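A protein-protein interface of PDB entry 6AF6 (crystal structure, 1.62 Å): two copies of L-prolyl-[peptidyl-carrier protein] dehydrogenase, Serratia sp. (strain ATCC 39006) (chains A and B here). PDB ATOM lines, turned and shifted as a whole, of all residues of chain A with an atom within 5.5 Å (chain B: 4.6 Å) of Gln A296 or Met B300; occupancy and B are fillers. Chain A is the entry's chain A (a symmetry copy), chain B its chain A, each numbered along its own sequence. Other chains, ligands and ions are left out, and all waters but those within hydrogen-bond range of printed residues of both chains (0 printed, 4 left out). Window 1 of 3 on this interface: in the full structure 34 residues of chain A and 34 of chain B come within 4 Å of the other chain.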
ATOM      1  N   LYS A 291     -16.406  27.647  -5.249  1.00  0.00           N
ATOM      2  CA  LYS A 291     -16.024  26.700  -6.296  1.00  0.00           C
ATOM      3  C   LYS A 291     -16.797  25.380  -6.187  1.00  0.00           C
ATOM      4  O   LYS A 291     -17.294  24.873  -7.205  1.00  0.00           O
ATOM      5  CB  LYS A 291     -14.511  26.464  -6.187  1.00  0.00           C
ATOM      6  CG  LYS A 291     -13.988  25.375  -7.152  1.00  0.00           C
ATOM      7  CD  LYS A 291     -14.053  25.813  -8.587  1.00  0.00           C
ATOM      8  CE  LYS A 291     -13.221  24.777  -9.418  1.00  0.00           C
ATOM      9  NZ  LYS A 291     -13.330  25.319 -10.807  1.00  0.00           N
ATOM     10  N   LEU A 292     -16.923  24.823  -4.986  1.00  0.00           N
ATOM     11  CA  LEU A 292     -17.683  23.560  -4.846  1.00  0.00           C
ATOM     12  C   LEU A 292     -19.124  23.754  -5.287  1.00  0.00           C
ATOM     13  O   LEU A 292     -19.687  22.877  -5.964  1.00  0.00           O
ATOM     14  CB  LEU A 292     -17.692  23.130  -3.384  1.00  0.00           C
ATOM     15  CG  LEU A 292     -16.331  22.686  -2.843  1.00  0.00           C
ATOM     16  CD1 LEU A 292     -16.426  22.601  -1.315  1.00  0.00           C
ATOM     17  CD2 LEU A 292     -15.948  21.351  -3.375  1.00  0.00           C
ATOM     18  N   ARG A 293     -19.739  24.876  -4.887  1.00  0.00           N
ATOM     19  CA  ARG A 293     -21.128  25.146  -5.314  1.00  0.00           C
ATOM     20  C   ARG A 293     -21.239  25.208  -6.823  1.00  0.00           C
ATOM     21  O   ARG A 293     -22.153  24.637  -7.430  1.00  0.00           O
ATOM     22  CB  ARG A 293     -21.605  26.503  -4.736  1.00  0.00           C
ATOM     23  CG  ARG A 293     -21.844  26.432  -3.248  1.00  0.00           C
ATOM     24  CD  ARG A 293     -22.082  27.879  -2.766  1.00  0.00           C
ATOM     25  NE  ARG A 293     -22.086  27.923  -1.328  1.00  0.00           N
ATOM     26  CZ  ARG A 293     -21.509  28.927  -0.654  1.00  0.00           C
ATOM     27  NH1 ARG A 293     -20.944  29.973  -1.318  1.00  0.00           N
ATOM     28  NH2 ARG A 293     -21.458  28.839   0.672  1.00  0.00           N
ATOM     29  N   LEU A 294     -20.315  25.931  -7.480  1.00  0.00           N
ATOM     30  CA  LEU A 294     -20.449  26.116  -8.904  1.00  0.00           C
ATOM     31  C   LEU A 294     -20.323  24.769  -9.636  1.00  0.00           C
ATOM     32  O   LEU A 294     -21.080  24.480 -10.574  1.00  0.00           O
ATOM     33  CB  LEU A 294     -19.347  27.090  -9.335  1.00  0.00           C
ATOM     34  CG  LEU A 294     -19.146  27.172 -10.859  1.00  0.00           C
ATOM     35  CD1 LEU A 294     -20.415  27.719 -11.564  1.00  0.00           C
ATOM     36  CD2 LEU A 294     -17.875  28.091 -11.215  1.00  0.00           C
ATOM     37  N   GLU A 295     -19.369  23.939  -9.217  1.00  0.00           N
ATOM     38  CA  GLU A 295     -19.160  22.674  -9.933  1.00  0.00           C
ATOM     39  C   GLU A 295     -20.362  21.767  -9.728  1.00  0.00           C
ATOM     40  O   GLU A 295     -20.834  21.125 -10.674  1.00  0.00           O
ATOM     41  CB  GLU A 295     -17.898  21.978  -9.422  1.00  0.00           C
ATOM     42  CG  GLU A 295     -16.634  22.828  -9.836  1.00  0.00           C
ATOM     43  CD  GLU A 295     -16.629  23.293 -11.335  1.00  0.00           C
ATOM     44  OE1 GLU A 295     -16.857  22.477 -12.263  1.00  0.00           O
ATOM     45  OE2 GLU A 295     -16.435  24.518 -11.598  1.00  0.00           O
ATOM     46  N   GLN A 296     -20.883  21.725  -8.494  1.00  0.00           N
ATOM     47  CA  GLN A 296     -22.012  20.816  -8.242  1.00  0.00           C
ATOM     48  C   GLN A 296     -23.254  21.255  -8.983  1.00  0.00           C
ATOM     49  O   GLN A 296     -23.941  20.442  -9.619  1.00  0.00           O
ATOM     50  CB  GLN A 296     -22.342  20.786  -6.744  1.00  0.00           C
ATOM     51  CG  GLN A 296     -21.335  20.007  -5.891  1.00  0.00           C
ATOM     52  CD  GLN A 296     -21.652  20.208  -4.447  1.00  0.00           C
ATOM     53  OE1 GLN A 296     -22.210  19.301  -3.796  1.00  0.00           O
ATOM     54  NE2 GLN A 296     -21.338  21.401  -3.898  1.00  0.00           N
ATOM     55  N   CYS A 297     -23.619  22.534  -8.866  1.00  0.00           N
ATOM     56  CA  CYS A 297     -24.892  22.924  -9.462  1.00  0.00           C
ATOM     57  C   CYS A 297     -24.818  22.951 -10.984  1.00  0.00           C
ATOM     58  O   CYS A 297     -25.817  22.652 -11.611  1.00  0.00           O
ATOM     59  CB  CYS A 297     -25.437  24.268  -8.926  1.00  0.00           C
ATOM     60  SG  CYS A 297     -24.560  25.758  -9.426  1.00  0.00           S
ATOM     61  N   ARG A 298     -23.663  23.224 -11.568  1.00  0.00           N
ATOM     62  CA  ARG A 298     -23.572  23.171 -13.027  1.00  0.00           C
ATOM     63  C   ARG A 298     -23.748  21.728 -13.515  1.00  0.00           C
ATOM     64  O   ARG A 298     -24.459  21.500 -14.494  1.00  0.00           O
ATOM     65  CB  ARG A 298     -22.266  23.825 -13.480  1.00  0.00           C
ATOM     66  CG  ARG A 298     -21.938  23.516 -14.919  1.00  0.00           C
ATOM     67  CD  ARG A 298     -21.023  24.574 -15.556  1.00  0.00           C
ATOM     68  NE  ARG A 298     -19.839  24.773 -14.763  1.00  0.00           N
ATOM     69  CZ  ARG A 298     -18.942  25.730 -14.929  1.00  0.00           C
ATOM     70  NH1 ARG A 298     -17.916  25.777 -14.096  1.00  0.00           N
ATOM     71  NH2 ARG A 298     -19.045  26.618 -15.894  1.00  0.00           N
ATOM     72  N   LEU A 299     -23.211  20.736 -12.776  1.00  0.00           N
ATOM     73  CA  LEU A 299     -23.430  19.349 -13.225  1.00  0.00           C
ATOM     74  C   LEU A 299     -24.893  18.965 -13.104  1.00  0.00           C
ATOM     75  O   LEU A 299     -25.426  18.229 -13.946  1.00  0.00           O
ATOM     76  CB  LEU A 299     -22.578  18.379 -12.385  1.00  0.00           C
ATOM     77  CG  LEU A 299     -21.116  18.457 -12.743  1.00  0.00           C
ATOM     78  CD1 LEU A 299     -20.298  17.674 -11.753  1.00  0.00           C
ATOM     79  CD2 LEU A 299     -20.848  17.971 -14.161  1.00  0.00           C
ATOM     80  N   MET A 300     -25.557  19.372 -12.005  1.00  0.00           N
ATOM     81  CA  MET A 300     -26.979  19.096 -11.846  1.00  0.00           C
ATOM     82  C   MET A 300     -27.794  19.686 -12.975  1.00  0.00           C
ATOM     83  O   MET A 300     -28.752  19.045 -13.452  1.00  0.00           O
ATOM     84  CB  MET A 300     -27.483  19.615 -10.497  1.00  0.00           C
ATOM     85  CG  MET A 300     -26.873  18.846  -9.308  1.00  0.00           C
ATOM     86  SD  MET A 300     -27.520  17.160  -9.103  1.00  0.00           S
ATOM     87  CE  MET A 300     -29.189  17.530  -8.530  1.00  0.00           C
ATOM     88  N   LEU A 301     -27.458  20.915 -13.392  1.00  0.00           N
ATOM     89  CA  LEU A 301     -28.200  21.565 -14.469  1.00  0.00           C
ATOM     90  C   LEU A 301     -27.969  20.824 -15.772  1.00  0.00           C
ATOM     91  O   LEU A 301     -28.931  20.520 -16.498  1.00  0.00           O
ATOM     92  CB  LEU A 301     -27.742  23.001 -14.637  1.00  0.00           C
ATOM     93  CG  LEU A 301     -28.518  23.719 -15.798  1.00  0.00           C
ATOM     94  CD1 LEU A 301     -29.952  23.737 -15.476  1.00  0.00           C
ATOM     95  CD2 LEU A 301     -27.955  25.081 -15.912  1.00  0.00           C
ATOM     96  N   TYR A 328     -27.214  28.709  -4.143  1.00  0.00           N
ATOM     97  CA  TYR A 328     -25.764  28.882  -4.245  1.00  0.00           C
ATOM     98  C   TYR A 328     -25.399  30.246  -4.802  1.00  0.00           C
ATOM     99  O   TYR A 328     -24.340  30.796  -4.430  1.00  0.00           O
ATOM    100  CB  TYR A 328     -25.171  27.785  -5.115  1.00  0.00           C
ATOM    101  CG  TYR A 328     -25.172  26.396  -4.548  1.00  0.00           C
ATOM    102  CD1 TYR A 328     -25.497  26.137  -3.206  1.00  0.00           C
ATOM    103  CD2 TYR A 328     -24.822  25.339  -5.381  1.00  0.00           C
ATOM    104  CE1 TYR A 328     -25.466  24.827  -2.718  1.00  0.00           C
ATOM    105  CE2 TYR A 328     -24.756  23.987  -4.877  1.00  0.00           C
ATOM    106  CZ  TYR A 328     -25.075  23.772  -3.554  1.00  0.00           C
ATOM    107  OH  TYR A 328     -25.053  22.514  -3.011  1.00  0.00           O
ATOM    108  N   GLN B 296     -25.585  15.359  -6.039  1.00  0.00           N
ATOM    109  CA  GLN B 296     -24.449  16.240  -6.348  1.00  0.00           C
ATOM    110  C   GLN B 296     -23.128  15.525  -6.173  1.00  0.00           C
ATOM    111  O   GLN B 296     -22.236  15.611  -7.030  1.00  0.00           O
ATOM    112  CB  GLN B 296     -24.455  17.456  -5.413  1.00  0.00           C
ATOM    113  CG  GLN B 296     -25.534  18.495  -5.732  1.00  0.00           C
ATOM    114  CD  GLN B 296     -25.566  19.524  -4.653  1.00  0.00           C
ATOM    115  OE1 GLN B 296     -25.070  20.652  -4.849  1.00  0.00           O
ATOM    116  NE2 GLN B 296     -26.118  19.174  -3.471  1.00  0.00           N
ATOM    117  N   CYS B 297     -22.937  14.859  -5.032  1.00  0.00           N
ATOM    118  CA  CYS B 297     -21.613  14.291  -4.804  1.00  0.00           C
ATOM    119  C   CYS B 297     -21.354  13.085  -5.699  1.00  0.00           C
ATOM    120  O   CYS B 297     -20.216  12.892  -6.083  1.00  0.00           O
ATOM    121  CB  CYS B 297     -21.346  13.929  -3.324  1.00  0.00           C
ATOM    122  SG  CYS B 297     -22.246  12.521  -2.656  1.00  0.00           S
ATOM    123  N   ARG B 298     -22.375  12.339  -6.086  1.00  0.00           N
ATOM    124  CA  ARG B 298     -22.138  11.230  -7.011  1.00  0.00           C
ATOM    125  C   ARG B 298     -21.706  11.769  -8.380  1.00  0.00           C
ATOM    126  O   ARG B 298     -20.777  11.227  -8.981  1.00  0.00           O
ATOM    127  CB  ARG B 298     -23.375  10.333  -7.059  1.00  0.00           C
ATOM    128  CG  ARG B 298     -23.345   9.373  -8.221  1.00  0.00           C
ATOM    129  CD  ARG B 298     -24.205   8.124  -7.979  1.00  0.00           C
ATOM    130  NE  ARG B 298     -25.549   8.488  -7.615  1.00  0.00           N
ATOM    131  CZ  ARG B 298     -26.485   7.668  -7.167  1.00  0.00           C
ATOM    132  NH1 ARG B 298     -27.667   8.176  -6.863  1.00  0.00           N
ATOM    133  NH2 ARG B 298     -26.268   6.379  -7.027  1.00  0.00           N
ATOM    134  N   LEU B 299     -22.283  12.902  -8.830  1.00  0.00           N
ATOM    135  CA  LEU B 299     -21.824  13.439 -10.124  1.00  0.00           C
ATOM    136  C   LEU B 299     -20.391  13.928 -10.029  1.00  0.00           C
ATOM    137  O   LEU B 299     -19.610  13.790 -10.981  1.00  0.00           O
ATOM    138  CB  LEU B 299     -22.730  14.603 -10.566  1.00  0.00           C
ATOM    139  CG  LEU B 299     -24.078  14.121 -11.038  1.00  0.00           C
ATOM    140  CD1 LEU B 299     -25.005  15.288 -11.239  1.00  0.00           C
ATOM    141  CD2 LEU B 299     -23.975  13.294 -12.313  1.00  0.00           C
ATOM    142  N   MET B 300     -20.031  14.599  -8.918  1.00  0.00           N
ATOM    143  CA  MET B 300     -18.657  15.046  -8.725  1.00  0.00           C
ATOM    144  C   MET B 300     -17.682  13.890  -8.757  1.00  0.00           C
ATOM    145  O   MET B 300     -16.581  14.021  -9.327  1.00  0.00           O
ATOM    146  CB  MET B 300     -18.520  15.823  -7.414  1.00  0.00           C
ATOM    147  CG  MET B 300     -19.290  17.158  -7.441  1.00  0.00           C
ATOM    148  SD  MET B 300     -18.528  18.436  -8.485  1.00  0.00           S
ATOM    149  CE  MET B 300     -17.074  18.828  -7.493  1.00  0.00           C
ATOM    150  N   LEU B 301     -18.048  12.766  -8.124  1.00  0.00           N
ATOM    151  CA  LEU B 301     -17.162  11.606  -8.095  1.00  0.00           C
ATOM    152  C   LEU B 301     -17.021  11.031  -9.492  1.00  0.00           C
ATOM    153  O   LEU B 301     -15.896  10.760  -9.945  1.00  0.00           O
ATOM    154  CB  LEU B 301     -17.723  10.533  -7.181  1.00  0.00           C
ATOM    155  CG  LEU B 301     -16.792   9.268  -7.141  1.00  0.00           C
ATOM    156  CD1 LEU B 301     -15.474   9.661  -6.622  1.00  0.00           C
ATOM    157  CD2 LEU B 301     -17.458   8.273  -6.276  1.00  0.00           C
ATOM    158  N   TYR B 302     -18.140  10.895 -10.182  1.00  0.00           N
ATOM    159  CA  TYR B 302     -18.097  10.322 -11.544  1.00  0.00           C
ATOM    160  C   TYR B 302     -17.255  11.183 -12.459  1.00  0.00           C
ATOM    161  O   TYR B 302     -16.446  10.672 -13.229  1.00  0.00           O
ATOM    162  CB  TYR B 302     -19.482  10.172 -12.127  1.00  0.00           C
ATOM    163  CG  TYR B 302     -20.351   9.150 -11.447  1.00  0.00           C
ATOM    164  CD1 TYR B 302     -19.850   8.227 -10.530  1.00  0.00           C
ATOM    165  CD2 TYR B 302     -21.696   9.108 -11.804  1.00  0.00           C
ATOM    166  CE1 TYR B 302     -20.704   7.311  -9.935  1.00  0.00           C
ATOM    167  CE2 TYR B 302     -22.535   8.165 -11.257  1.00  0.00           C
ATOM    168  CZ  TYR B 302     -22.005   7.257 -10.338  1.00  0.00           C
ATOM    169  OH  TYR B 302     -22.847   6.326  -9.773  1.00  0.00           O
ATOM    170  N   ARG B 303     -17.388  12.497 -12.360  1.00  0.00           N
ATOM    171  CA  ARG B 303     -16.573  13.312 -13.248  1.00  0.00           C
ATOM    172  C   ARG B 303     -15.104  13.241 -12.881  1.00  0.00           C
ATOM    173  O   ARG B 303     -14.253  13.231 -13.776  1.00  0.00           O
ATOM    174  CB  ARG B 303     -17.043  14.769 -13.245  1.00  0.00           C
ATOM    175  CG  ARG B 303     -16.243  15.606 -14.197  1.00  0.00           C
ATOM    176  CD  ARG B 303     -16.872  16.976 -14.296  1.00  0.00           C
ATOM    177  NE  ARG B 303     -16.515  17.743 -13.124  1.00  0.00           N
ATOM    178  CZ  ARG B 303     -16.801  19.036 -12.949  1.00  0.00           C
ATOM    179  NH1 ARG B 303     -17.461  19.699 -13.878  1.00  0.00           N
ATOM    180  NH2 ARG B 303     -16.426  19.660 -11.847  1.00  0.00           N
ATOM    181  N   ALA B 304     -14.758  13.214 -11.578  1.00  0.00           N
ATOM    182  CA  ALA B 304     -13.369  13.132 -11.163  1.00  0.00           C
ATOM    183  C   ALA B 304     -12.744  11.857 -11.712  1.00  0.00           C
ATOM    184  O   ALA B 304     -11.641  11.883 -12.288  1.00  0.00           O
ATOM    185  CB  ALA B 304     -13.234  13.140  -9.642  1.00  0.00           C
ATOM    186  N   MET B 320     -12.118  17.528  -4.203  1.00  0.00           N
ATOM    187  CA  MET B 320     -13.476  18.082  -4.021  1.00  0.00           C
ATOM    188  C   MET B 320     -14.481  16.981  -3.764  1.00  0.00           C
ATOM    189  O   MET B 320     -15.367  17.122  -2.903  1.00  0.00           O
ATOM    190  CB  MET B 320     -13.952  18.866  -5.248  1.00  0.00           C
ATOM    191  CG  MET B 320     -13.147  20.143  -5.426  1.00  0.00           C
ATOM    192  SD  MET B 320     -13.893  21.192  -6.729  1.00  0.00           S
ATOM    193  CE  MET B 320     -13.522  20.365  -8.231  1.00  0.00           C
ATOM    194  N   SER B 321     -14.341  15.856  -4.496  1.00  0.00           N
ATOM    195  CA  SER B 321     -15.253  14.733  -4.301  1.00  0.00           C
ATOM    196  C   SER B 321     -15.114  14.148  -2.913  1.00  0.00           C
ATOM    197  O   SER B 321     -16.126  13.830  -2.256  1.00  0.00           O
ATOM    198  CB  SER B 321     -14.959  13.673  -5.378  1.00  0.00           C
ATOM    199  OG  SER B 321     -15.330  14.228  -6.612  1.00  0.00           O
ATOM    200  N   LEU B 324     -16.738  16.507  -0.362  1.00  0.00           N
ATOM    201  CA  LEU B 324     -18.195  16.568  -0.361  1.00  0.00           C
ATOM    202  C   LEU B 324     -18.785  15.260   0.102  1.00  0.00           C
ATOM    203  O   LEU B 324     -19.745  15.257   0.899  1.00  0.00           O
ATOM    204  CB  LEU B 324     -18.713  16.876  -1.744  1.00  0.00           C
ATOM    205  CG  LEU B 324     -18.371  18.288  -2.237  1.00  0.00           C
ATOM    206  CD1 LEU B 324     -18.689  18.287  -3.720  1.00  0.00           C
ATOM    207  CD2 LEU B 324     -19.199  19.332  -1.484  1.00  0.00           C
ATOM    208  N   TYR B 328     -21.147  15.067   3.341  1.00  0.00           N
ATOM    209  CA  TYR B 328     -22.549  14.724   3.097  1.00  0.00           C
ATOM    210  C   TYR B 328     -22.927  13.405   3.745  1.00  0.00           C
ATOM    211  O   TYR B 328     -24.094  13.238   4.160  1.00  0.00           O
ATOM    212  CB  TYR B 328     -22.816  14.669   1.601  1.00  0.00           C
ATOM    213  CG  TYR B 328     -22.791  15.973   0.859  1.00  0.00           C
ATOM    214  CD1 TYR B 328     -22.743  17.209   1.523  1.00  0.00           C
ATOM    215  CD2 TYR B 328     -22.834  15.946  -0.530  1.00  0.00           C
ATOM    216  CE1 TYR B 328     -22.740  18.399   0.790  1.00  0.00           C
ATOM    217  CE2 TYR B 328     -22.865  17.171  -1.295  1.00  0.00           C
ATOM    218  CZ  TYR B 328     -22.822  18.365  -0.609  1.00  0.00           C
ATOM    219  OH  TYR B 328     -22.829  19.567  -1.268  1.00  0.00           O
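Of the 12 printed residues of chain A, 6 touch a printed residue of chain B. Along chain A the printed residues that touch a printed residue of chain B span positions 292 to 328. Of the 13 printed residues of chain B, 7 touch a printed residue of chain A.
Gln B296 touches its own counterpart, Gln A296. Gln A296 touches Met B300, and with the chains exchanged Met A300 touches Gln B296. Gln A296 touches Tyr B328, and with the chains exchanged Tyr A328 touches Gln B296. Leu A299 touches Met B300, and with the chains exchanged Met A300 touches Leu B299. Positions printed for both chains: 296, 297, 298, 299, 300, 301 and 328. Of the 12 pairs that touch across the chains among the printed residues, 7 have their exchanged pair printed and touching as well.
The side-chain amide oxygen (OE1) of Gln A296 lies close to the side-chain amide oxygen (OE1) of Gln B296 (3.3 Å). The side-chain hydroxyl of Tyr A328 lies within hydrogen-bond range of the side-chain amide oxygen of Gln B296 (2.6 Å). NH2 of Arg B303 is in salt-bridge range of OE1 of Glu A295 (2.9 Å). The side-chain amide oxygen of Gln A296 sits at hydrogen-bond distance from the side-chain hydroxyl of Tyr B328, 2.6 Å away.
Gln A296 touches just these residues of chain B: Gln B296, Met B300, Leu B324 and Tyr B328. Of the printed residues of chain B, Leu A299 touches Met B300 and Arg B303. Printed residues of chain A within 4 Å of Gln B296: Gln A296, Met A300 and Tyr A328. Cys B297 touches none of the printed residues of chain A. Arg A293 touches none of the printed residues of chain B. The nearest printed residue of chain A that does not touch Met B320 is Lys A291 (4.2 Å).
The side-chain hydroxyl (OG) of Ser B321 is in hydrogen-bond range of the backbone carbonyl oxygen (O) of Met B300 (3.0 Å). NZ of Lys A291 is in salt-bridge range of OE2 of Glu A295 (3.3 Å). The side-chain amide nitrogen (NE2) of Gln A296 is in hydrogen-bond range of the backbone carbonyl oxygen (O) of Leu A292, 3.0 Å away. The guanidinium group (NH1) of Arg A298 lies within salt-bridge range of the side-chain carboxylate (OE2) of Glu A295.
Among the printed residues, merely in contact across the chains: Leu A292 with Met B320 (3.7 Å), Glu A295 with Met B300 (3.7 Å), Gln A296 with Met B300 (3.8 Å), Gln A296 with Leu B324 (3.6 Å), Leu A299 with Met B300 (3.8 Å), Leu A299 with Arg B303 (3.8 Å), Met A300 with Gln B296 (3.8 Å) and Met A300 with Leu B299 (3.8 Å).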
